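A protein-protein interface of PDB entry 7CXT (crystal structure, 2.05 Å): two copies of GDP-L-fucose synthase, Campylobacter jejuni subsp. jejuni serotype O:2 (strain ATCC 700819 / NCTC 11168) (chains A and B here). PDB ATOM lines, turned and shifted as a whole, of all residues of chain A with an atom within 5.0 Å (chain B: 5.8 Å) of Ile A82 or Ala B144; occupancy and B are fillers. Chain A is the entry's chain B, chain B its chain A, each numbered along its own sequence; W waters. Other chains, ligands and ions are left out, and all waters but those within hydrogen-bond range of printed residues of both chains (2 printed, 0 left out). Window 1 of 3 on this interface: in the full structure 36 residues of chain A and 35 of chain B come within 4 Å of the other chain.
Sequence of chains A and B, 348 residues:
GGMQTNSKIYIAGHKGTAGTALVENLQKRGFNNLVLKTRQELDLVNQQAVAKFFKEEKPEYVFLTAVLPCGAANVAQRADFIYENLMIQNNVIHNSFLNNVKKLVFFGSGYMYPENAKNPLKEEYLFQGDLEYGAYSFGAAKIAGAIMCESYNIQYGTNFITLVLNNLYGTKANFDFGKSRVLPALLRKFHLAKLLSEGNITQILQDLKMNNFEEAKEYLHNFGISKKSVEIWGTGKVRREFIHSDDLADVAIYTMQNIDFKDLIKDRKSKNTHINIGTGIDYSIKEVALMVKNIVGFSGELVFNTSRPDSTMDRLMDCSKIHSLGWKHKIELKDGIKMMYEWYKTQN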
ATOM      1  N   ARG A  78     -25.513 -11.527 -14.301  1.00  0.00           N
ATOM      2  CA  ARG A  78     -26.633 -11.323 -15.218  1.00  0.00           C
ATOM      3  C   ARG A  78     -26.252 -10.422 -16.389  1.00  0.00           C
ATOM      4  O   ARG A  78     -26.706 -10.640 -17.524  1.00  0.00           O
ATOM      5  CB  ARG A  78     -27.814 -10.726 -14.438  1.00  0.00           C
ATOM      6  CG  ARG A  78     -29.149 -10.667 -15.168  1.00  0.00           C
ATOM      7  CD  ARG A  78     -30.230 -10.318 -14.138  1.00  0.00           C
ATOM      8  NE  ARG A  78     -31.586 -10.507 -14.633  1.00  0.00           N
ATOM      9  CZ  ARG A  78     -32.258 -11.648 -14.540  1.00  0.00           C
ATOM     10  NH1 ARG A  78     -31.682 -12.707 -13.985  1.00  0.00           N
ATOM     11  NH2 ARG A  78     -33.505 -11.724 -15.005  1.00  0.00           N
ATOM     12  N   ALA A  79     -25.400  -9.420 -16.143  1.00  0.00           N
ATOM     13  CA  ALA A  79     -24.956  -8.545 -17.229  1.00  0.00           C
ATOM     14  C   ALA A  79     -23.914  -9.223 -18.119  1.00  0.00           C
ATOM     15  O   ALA A  79     -23.960  -9.081 -19.348  1.00  0.00           O
ATOM     16  CB  ALA A  79     -24.378  -7.239 -16.661  1.00  0.00           C
ATOM     17  N   ASP A  80     -22.968  -9.959 -17.522  1.00  0.00           N
ATOM     18  CA  ASP A  80     -21.929 -10.608 -18.323  1.00  0.00           C
ATOM     19  C   ASP A  80     -22.533 -11.637 -19.277  1.00  0.00           C
ATOM     20  O   ASP A  80     -22.052 -11.792 -20.410  1.00  0.00           O
ATOM     21  CB  ASP A  80     -20.896 -11.269 -17.408  1.00  0.00           C
ATOM     22  CG  ASP A  80     -20.332 -10.318 -16.364  1.00  0.00           C
ATOM     23  OD1 ASP A  80     -20.342  -9.078 -16.586  1.00  0.00           O
ATOM     24  OD2 ASP A  80     -19.895 -10.820 -15.309  1.00  0.00           O
ATOM     25  N   PHE A  81     -23.621 -12.289 -18.862  1.00  0.00           N
ATOM     26  CA  PHE A  81     -24.268 -13.303 -19.688  1.00  0.00           C
ATOM     27  C   PHE A  81     -24.748 -12.725 -21.010  1.00  0.00           C
ATOM     28  O   PHE A  81     -24.645 -13.382 -22.050  1.00  0.00           O
ATOM     29  CB  PHE A  81     -25.461 -13.919 -18.950  1.00  0.00           C
ATOM     30  CG  PHE A  81     -25.081 -14.852 -17.838  1.00  0.00           C
ATOM     31  CD1 PHE A  81     -24.015 -15.728 -17.985  1.00  0.00           C
ATOM     32  CD2 PHE A  81     -25.795 -14.851 -16.636  1.00  0.00           C
ATOM     33  CE1 PHE A  81     -23.651 -16.589 -16.948  1.00  0.00           C
ATOM     34  CE2 PHE A  81     -25.443 -15.711 -15.595  1.00  0.00           C
ATOM     35  CZ  PHE A  81     -24.364 -16.586 -15.758  1.00  0.00           C
ATOM     36  N   ILE A  82     -25.308 -11.516 -20.999  1.00  0.00           N
ATOM     37  CA  ILE A  82     -25.812 -11.019 -22.271  1.00  0.00           C
ATOM     38  C   ILE A  82     -24.725 -10.263 -23.026  1.00  0.00           C
ATOM     39  O   ILE A  82     -24.503 -10.526 -24.206  1.00  0.00           O
ATOM     40  CB  ILE A  82     -27.117 -10.198 -22.090  1.00  0.00           C
ATOM     41  CG1 ILE A  82     -27.598  -9.662 -23.445  1.00  0.00           C
ATOM     42  CG2 ILE A  82     -26.979  -9.074 -21.051  1.00  0.00           C
ATOM     43  CD1 ILE A  82     -29.006  -9.077 -23.453  1.00  0.00           C
ATOM     44  N   TYR A  83     -23.934  -9.415 -22.362  1.00  0.00           N
ATOM     45  CA  TYR A  83     -22.884  -8.696 -23.090  1.00  0.00           C
ATOM     46  C   TYR A  83     -21.851  -9.653 -23.691  1.00  0.00           C
ATOM     47  O   TYR A  83     -21.593  -9.621 -24.900  1.00  0.00           O
ATOM     48  CB  TYR A  83     -22.190  -7.674 -22.181  1.00  0.00           C
ATOM     49  CG  TYR A  83     -20.977  -7.063 -22.857  1.00  0.00           C
ATOM     50  CD1 TYR A  83     -21.129  -6.195 -23.924  1.00  0.00           C
ATOM     51  CD2 TYR A  83     -19.678  -7.384 -22.453  1.00  0.00           C
ATOM     52  CE1 TYR A  83     -20.038  -5.648 -24.566  1.00  0.00           C
ATOM     53  CE2 TYR A  83     -18.568  -6.845 -23.101  1.00  0.00           C
ATOM     54  CZ  TYR A  83     -18.760  -5.970 -24.161  1.00  0.00           C
ATOM     55  OH  TYR A  83     -17.685  -5.411 -24.839  1.00  0.00           O
ATOM     56  N   GLU A  84     -21.272 -10.541 -22.875  1.00  0.00           N
ATOM     57  CA  GLU A  84     -20.190 -11.382 -23.392  1.00  0.00           C
ATOM     58  C   GLU A  84     -20.668 -12.344 -24.476  1.00  0.00           C
ATOM     59  O   GLU A  84     -19.982 -12.530 -25.492  1.00  0.00           O
ATOM     60  CB  GLU A  84     -19.519 -12.148 -22.249  1.00  0.00           C
ATOM     61  CG  GLU A  84     -18.738 -11.214 -21.342  1.00  0.00           C
ATOM     62  CD  GLU A  84     -17.931 -11.928 -20.286  1.00  0.00           C
ATOM     63  OE1 GLU A  84     -17.551 -13.098 -20.496  1.00  0.00           O
ATOM     64  OE2 GLU A  84     -17.675 -11.310 -19.238  1.00  0.00           O
ATOM     65  N   ASN A  85     -21.832 -12.972 -24.291  1.00  0.00           N
ATOM     66  CA  ASN A  85     -22.288 -13.907 -25.317  1.00  0.00           C
ATOM     67  C   ASN A  85     -22.732 -13.186 -26.585  1.00  0.00           C
ATOM     68  O   ASN A  85     -22.494 -13.680 -27.687  1.00  0.00           O
ATOM     69  CB  ASN A  85     -23.392 -14.797 -24.766  1.00  0.00           C
ATOM     70  CG  ASN A  85     -22.860 -15.812 -23.792  1.00  0.00           C
ATOM     71  OD1 ASN A  85     -21.886 -16.497 -24.091  1.00  0.00           O
ATOM     72  ND2 ASN A  85     -23.472 -15.900 -22.606  1.00  0.00           N
ATOM     73  N   LEU A  86     -23.345 -12.002 -26.456  1.00  0.00           N
ATOM     74  CA  LEU A  86     -23.696 -11.222 -27.640  1.00  0.00           C
ATOM     75  C   LEU A  86     -22.448 -10.812 -28.416  1.00  0.00           C
ATOM     76  O   LEU A  86     -22.428 -10.861 -29.649  1.00  0.00           O
ATOM     77  CB  LEU A  86     -24.494  -9.970 -27.244  1.00  0.00           C
ATOM     78  CG  LEU A  86     -25.990 -10.062 -26.919  1.00  0.00           C
ATOM     79  CD1 LEU A  86     -26.625  -8.639 -26.685  1.00  0.00           C
ATOM     80  CD2 LEU A  86     -26.668 -10.789 -28.038  1.00  0.00           C
ATOM     81  N   MET A  87     -21.386 -10.433 -27.704  1.00  0.00           N
ATOM     82  CA  MET A  87     -20.179  -9.991 -28.386  1.00  0.00           C
ATOM     83  C   MET A  87     -19.508 -11.164 -29.091  1.00  0.00           C
ATOM     84  O   MET A  87     -19.160 -11.066 -30.272  1.00  0.00           O
ATOM     85  CB  MET A  87     -19.224  -9.320 -27.400  1.00  0.00           C
ATOM     86  CG  MET A  87     -19.640  -7.919 -26.930  1.00  0.00           C
ATOM     87  SD  MET A  87     -19.932  -6.656 -28.188  1.00  0.00           S
ATOM     88  CE  MET A  87     -18.329  -6.566 -29.004  1.00  0.00           C
ATOM     89  N   SER A 137     -31.280 -13.263 -19.073  1.00  0.00           N
ATOM     90  CA  SER A 137     -30.422 -12.505 -19.976  1.00  0.00           C
ATOM     91  C   SER A 137     -29.572 -13.433 -20.826  1.00  0.00           C
ATOM     92  O   SER A 137     -29.262 -13.098 -21.973  1.00  0.00           O
ATOM     93  CB  SER A 137     -29.558 -11.498 -19.193  1.00  0.00           C
ATOM     94  OG  SER A 137     -28.583 -12.140 -18.377  1.00  0.00           O
ATOM     95  N   ALA A 140     -31.924 -14.556 -23.547  1.00  0.00           N
ATOM     96  CA  ALA A 140     -32.089 -13.486 -24.518  1.00  0.00           C
ATOM     97  C   ALA A 140     -30.884 -13.404 -25.443  1.00  0.00           C
ATOM     98  O   ALA A 140     -31.035 -13.221 -26.651  1.00  0.00           O
ATOM     99  CB  ALA A 140     -32.314 -12.154 -23.807  1.00  0.00           C
ATOM    100  N   ALA A 141     -29.680 -13.568 -24.898  1.00  0.00           N
ATOM    101  CA  ALA A 141     -28.493 -13.588 -25.747  1.00  0.00           C
ATOM    102  C   ALA A 141     -28.561 -14.725 -26.751  1.00  0.00           C
ATOM    103  O   ALA A 141     -28.264 -14.537 -27.942  1.00  0.00           O
ATOM    104  CB  ALA A 141     -27.227 -13.719 -24.890  1.00  0.00           C
ATOM    105  N   LEU B  86     -27.207  -4.151 -32.394  1.00  0.00           N
ATOM    106  CA  LEU B  86     -26.637  -4.819 -31.227  1.00  0.00           C
ATOM    107  C   LEU B  86     -25.238  -4.300 -30.927  1.00  0.00           C
ATOM    108  O   LEU B  86     -24.856  -4.171 -29.759  1.00  0.00           O
ATOM    109  CB  LEU B  86     -26.573  -6.337 -31.427  1.00  0.00           C
ATOM    110  CG  LEU B  86     -27.839  -7.158 -31.338  1.00  0.00           C
ATOM    111  CD1 LEU B  86     -27.539  -8.666 -31.481  1.00  0.00           C
ATOM    112  CD2 LEU B  86     -28.588  -6.831 -30.020  1.00  0.00           C
ATOM    113  N   GLN B  89     -25.485  -0.790 -29.401  1.00  0.00           N
ATOM    114  CA  GLN B  89     -25.985  -0.909 -28.034  1.00  0.00           C
ATOM    115  C   GLN B  89     -24.924  -1.490 -27.116  1.00  0.00           C
ATOM    116  O   GLN B  89     -24.624  -0.912 -26.067  1.00  0.00           O
ATOM    117  CB  GLN B  89     -27.244  -1.775 -28.001  1.00  0.00           C
ATOM    118  CG  GLN B  89     -28.429  -1.163 -28.722  1.00  0.00           C
ATOM    119  CD  GLN B  89     -29.445  -2.201 -29.166  1.00  0.00           C
ATOM    120  OE1 GLN B  89     -29.404  -3.367 -28.744  1.00  0.00           O
ATOM    121  NE2 GLN B  89     -30.373  -1.777 -30.017  1.00  0.00           N
ATOM    122  N   ASN B  90     -24.308  -2.612 -27.521  1.00  0.00           N
ATOM    123  CA  ASN B  90     -23.298  -3.247 -26.678  1.00  0.00           C
ATOM    124  C   ASN B  90     -22.114  -2.322 -26.445  1.00  0.00           C
ATOM    125  O   ASN B  90     -21.667  -2.147 -25.306  1.00  0.00           O
ATOM    126  CB  ASN B  90     -22.797  -4.532 -27.317  1.00  0.00           C
ATOM    127  CG  ASN B  90     -23.827  -5.604 -27.344  1.00  0.00           C
ATOM    128  OD1 ASN B  90     -24.959  -5.412 -26.904  1.00  0.00           O
ATOM    129  ND2 ASN B  90     -23.449  -6.756 -27.869  1.00  0.00           N
ATOM    130  N   GLY B 139     -36.554  -5.763 -33.947  1.00  0.00           N
ATOM    131  CA  GLY B 139     -37.178  -5.793 -32.638  1.00  0.00           C
ATOM    132  C   GLY B 139     -36.401  -6.639 -31.655  1.00  0.00           C
ATOM    133  O   GLY B 139     -36.229  -6.254 -30.496  1.00  0.00           O
ATOM    134  N   ALA B 140     -35.841  -7.763 -32.126  1.00  0.00           N
ATOM    135  CA  ALA B 140     -35.024  -8.593 -31.246  1.00  0.00           C
ATOM    136  C   ALA B 140     -33.783  -7.839 -30.764  1.00  0.00           C
ATOM    137  O   ALA B 140     -33.363  -7.988 -29.613  1.00  0.00           O
ATOM    138  CB  ALA B 140     -34.611  -9.879 -31.974  1.00  0.00           C
ATOM    139  N   ALA B 141     -33.178  -7.030 -31.626  1.00  0.00           N
ATOM    140  CA  ALA B 141     -32.049  -6.211 -31.180  1.00  0.00           C
ATOM    141  C   ALA B 141     -32.484  -5.174 -30.138  1.00  0.00           C
ATOM    142  O   ALA B 141     -31.754  -4.905 -29.174  1.00  0.00           O
ATOM    143  CB  ALA B 141     -31.412  -5.514 -32.386  1.00  0.00           C
ATOM    144  N   LYS B 142     -33.667  -4.575 -30.317  1.00  0.00           N
ATOM    145  CA  LYS B 142     -34.154  -3.614 -29.326  1.00  0.00           C
ATOM    146  C   LYS B 142     -34.474  -4.296 -28.002  1.00  0.00           C
ATOM    147  O   LYS B 142     -34.248  -3.720 -26.934  1.00  0.00           O
ATOM    148  CB  LYS B 142     -35.389  -2.878 -29.849  1.00  0.00           C
ATOM    149  CG  LYS B 142     -35.074  -1.779 -30.855  1.00  0.00           C
ATOM    150  CD  LYS B 142     -34.258  -0.665 -30.220  1.00  0.00           C
ATOM    151  CE  LYS B 142     -33.957   0.424 -31.253  1.00  0.00           C
ATOM    152  NZ  LYS B 142     -33.059   1.499 -30.728  1.00  0.00           N
ATOM    153  N   ILE B 143     -34.945  -5.541 -28.050  1.00  0.00           N
ATOM    154  CA  ILE B 143     -35.170  -6.283 -26.815  1.00  0.00           C
ATOM    155  C   ILE B 143     -33.853  -6.468 -26.078  1.00  0.00           C
ATOM    156  O   ILE B 143     -33.756  -6.240 -24.864  1.00  0.00           O
ATOM    157  CB  ILE B 143     -35.849  -7.632 -27.136  1.00  0.00           C
ATOM    158  CG1 ILE B 143     -37.302  -7.399 -27.596  1.00  0.00           C
ATOM    159  CG2 ILE B 143     -35.742  -8.607 -25.946  1.00  0.00           C
ATOM    160  CD1 ILE B 143     -38.054  -8.672 -28.013  1.00  0.00           C
ATOM    161  N   ALA B 144     -32.809  -6.850 -26.810  1.00  0.00           N
ATOM    162  CA  ALA B 144     -31.523  -7.098 -26.183  1.00  0.00           C
ATOM    163  C   ALA B 144     -30.941  -5.825 -25.588  1.00  0.00           C
ATOM    164  O   ALA B 144     -30.261  -5.883 -24.561  1.00  0.00           O
ATOM    165  CB  ALA B 144     -30.549  -7.713 -27.203  1.00  0.00           C
ATOM    166  N   GLY B 145     -31.209  -4.673 -26.194  1.00  0.00           N
ATOM    167  CA  GLY B 145     -30.761  -3.428 -25.589  1.00  0.00           C
ATOM    168  C   GLY B 145     -31.471  -3.145 -24.279  1.00  0.00           C
ATOM    169  O   GLY B 145     -30.842  -2.757 -23.290  1.00  0.00           O
ATOM    170  N   ALA B 146     -32.781  -3.416 -24.230  1.00  0.00           N
ATOM    171  CA  ALA B 146     -33.522  -3.192 -22.996  1.00  0.00           C
ATOM    172  C   ALA B 146     -33.060  -4.159 -21.914  1.00  0.00           C
ATOM    173  O   ALA B 146     -32.760  -3.738 -20.794  1.00  0.00           O
ATOM    174  CB  ALA B 146     -35.027  -3.313 -23.256  1.00  0.00           C
ATOM    175  N   ILE B 147     -32.898  -5.439 -22.256  1.00  0.00           N
ATOM    176  CA  ILE B 147     -32.437  -6.411 -21.271  1.00  0.00           C
ATOM    177  C   ILE B 147     -31.008  -6.124 -20.816  1.00  0.00           C
ATOM    178  O   ILE B 147     -30.677  -6.329 -19.643  1.00  0.00           O
ATOM    179  CB  ILE B 147     -32.608  -7.831 -21.849  1.00  0.00           C
ATOM    180  CG1 ILE B 147     -34.128  -8.129 -21.936  1.00  0.00           C
ATOM    181  CG2 ILE B 147     -31.898  -8.865 -20.979  1.00  0.00           C
ATOM    182  CD1 ILE B 147     -34.486  -9.488 -22.591  1.00  0.00           C
ATOM    183  N   MET B 148     -30.152  -5.618 -21.709  1.00  0.00           N
ATOM    184  CA  MET B 148     -28.785  -5.267 -21.325  1.00  0.00           C
ATOM    185  C   MET B 148     -28.769  -4.182 -20.254  1.00  0.00           C
ATOM    186  O   MET B 148     -28.105  -4.326 -19.218  1.00  0.00           O
ATOM    187  CB  MET B 148     -28.001  -4.780 -22.551  1.00  0.00           C
ATOM    188  CG  MET B 148     -27.386  -5.873 -23.388  1.00  0.00           C
ATOM    189  SD  MET B 148     -25.622  -5.989 -23.081  1.00  0.00           S
ATOM    190  CE  MET B 148     -25.160  -4.295 -23.462  1.00  0.00           C
ATOM    191  N   CYS B 149     -29.515  -3.091 -20.488  1.00  0.00           N
ATOM    192  CA  CYS B 149     -29.619  -2.020 -19.495  1.00  0.00           C
ATOM    193  C   CYS B 149     -30.046  -2.573 -18.147  1.00  0.00           C
ATOM    194  O   CYS B 149     -29.427  -2.289 -17.114  1.00  0.00           O
ATOM    195  CB  CYS B 149     -30.633  -0.967 -19.945  1.00  0.00           C
ATOM    196  SG  CYS B 149     -30.184   0.053 -21.352  1.00  0.00           S
ATOM    197  N   SER B 151     -29.881  -5.659 -17.078  1.00  0.00           N
ATOM    198  CA  SER B 151     -28.931  -6.619 -16.529  1.00  0.00           C
ATOM    199  C   SER B 151     -27.731  -5.916 -15.912  1.00  0.00           C
ATOM    200  O   SER B 151     -27.197  -6.373 -14.894  1.00  0.00           O
ATOM    201  CB  SER B 151     -28.506  -7.613 -17.616  1.00  0.00           C
ATOM    202  OG  SER B 151     -29.650  -8.354 -18.038  1.00  0.00           O
ATOM    203  N   TYR B 152     -27.308  -4.790 -16.493  1.00  0.00           N
ATOM    204  CA  TYR B 152     -26.238  -4.013 -15.869  1.00  0.00           C
ATOM    205  C   TYR B 152     -26.713  -3.331 -14.593  1.00  0.00           C
ATOM    206  O   TYR B 152     -25.959  -3.240 -13.617  1.00  0.00           O
ATOM    207  CB  TYR B 152     -25.671  -2.993 -16.860  1.00  0.00           C
ATOM    208  CG  TYR B 152     -24.573  -3.589 -17.743  1.00  0.00           C
ATOM    209  CD1 TYR B 152     -24.894  -4.365 -18.852  1.00  0.00           C
ATOM    210  CD2 TYR B 152     -23.220  -3.394 -17.447  1.00  0.00           C
ATOM    211  CE1 TYR B 152     -23.906  -4.920 -19.650  1.00  0.00           C
ATOM    212  CE2 TYR B 152     -22.209  -3.942 -18.257  1.00  0.00           C
ATOM    213  CZ  TYR B 152     -22.570  -4.704 -19.348  1.00  0.00           C
ATOM    214  OH  TYR B 152     -21.610  -5.277 -20.141  1.00  0.00           O
HETATM  215  O   HOH W   1     -20.454  -7.532 -18.993  1.00  0.00           O
HETATM  216  O   HOH W   2     -32.302  -8.580 -16.625  1.00  0.00           O
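ND2 of Asn B90 is in hydrogen-bond range of SD of Met A87.
The backbone carbonyl oxygen of Leu B86 sits close to the side-chain amide oxygen of Asn B90, at 3.1 Å. The side-chain hydroxyl of Ser B151 lies within hydrogen-bond range of the backbone carbonyl oxygen of Ile B147, 2.8 Å away. The side-chain hydroxyl of Ser A137 lies within hydrogen-bond range of the backbone carbonyl oxygen of Arg A78, at 2.5 Å.
Arg A78 touches Ser B151 (O to CB, 3.5 Å). CB of Ala A79 touches O of Ser B151, 3.4 Å away. Ala A79 touches Tyr B152 (CB to CD1, 3.7 Å). Ile A82 touches Ala B144. Ile B147 touches Ile A82. Ile A82 touches Met B148 (CD1 to CG, 3.6 Å). Tyr A83 touches Met B148. CB of Leu A86 touches ND2 of Asn B90, 3.4 Å away. CB of Ser A137 touches OG of Ser B151 (3.4 Å). CB of Ala A140 touches CD1 of Ile B147 (3.6 Å).
Glu A84 touches none of the printed residues of chain B. Printed residues of chain B within 4 Å of Ser A137: Ile B147 (3.9 Å) and Ser B151 (3.4 Å). Of the printed residues of chain B, Ala A140 touches Ile B147 (3.6 Å). Ala B144 touches just one residue of chain A: Ile A82 (3.6 Å). The nearest residue of chain A that does not touch Ala B144 is Leu A86 (4.1 Å).
Of the 16 printed residues of chain B, 6 touch a printed residue of chain A. Hydrophobic or aromatic side chains of chain B that line the printed part of chain A: Ile B147, Met B148 and Tyr B152. Along chain B the printed residues that touch a printed residue of chain A span positions 90 to 152.
3 positions are printed for both chains. Of the 14 pairs that touch across the chains among the printed residues, none has its exchanged pair printed and touching as well.
Water W1 lies within hydrogen-bond range of the side-chain hydroxyl (OH) of Tyr B152 and the side-chain carboxylate (OD1) of Asp A80. Water W2 lies within hydrogen-bond range of the guanidinium group (NE) of Arg A78 (2.9 Å) and the side-chain hydroxyl (OG) of Ser B151 (3.0 Å).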
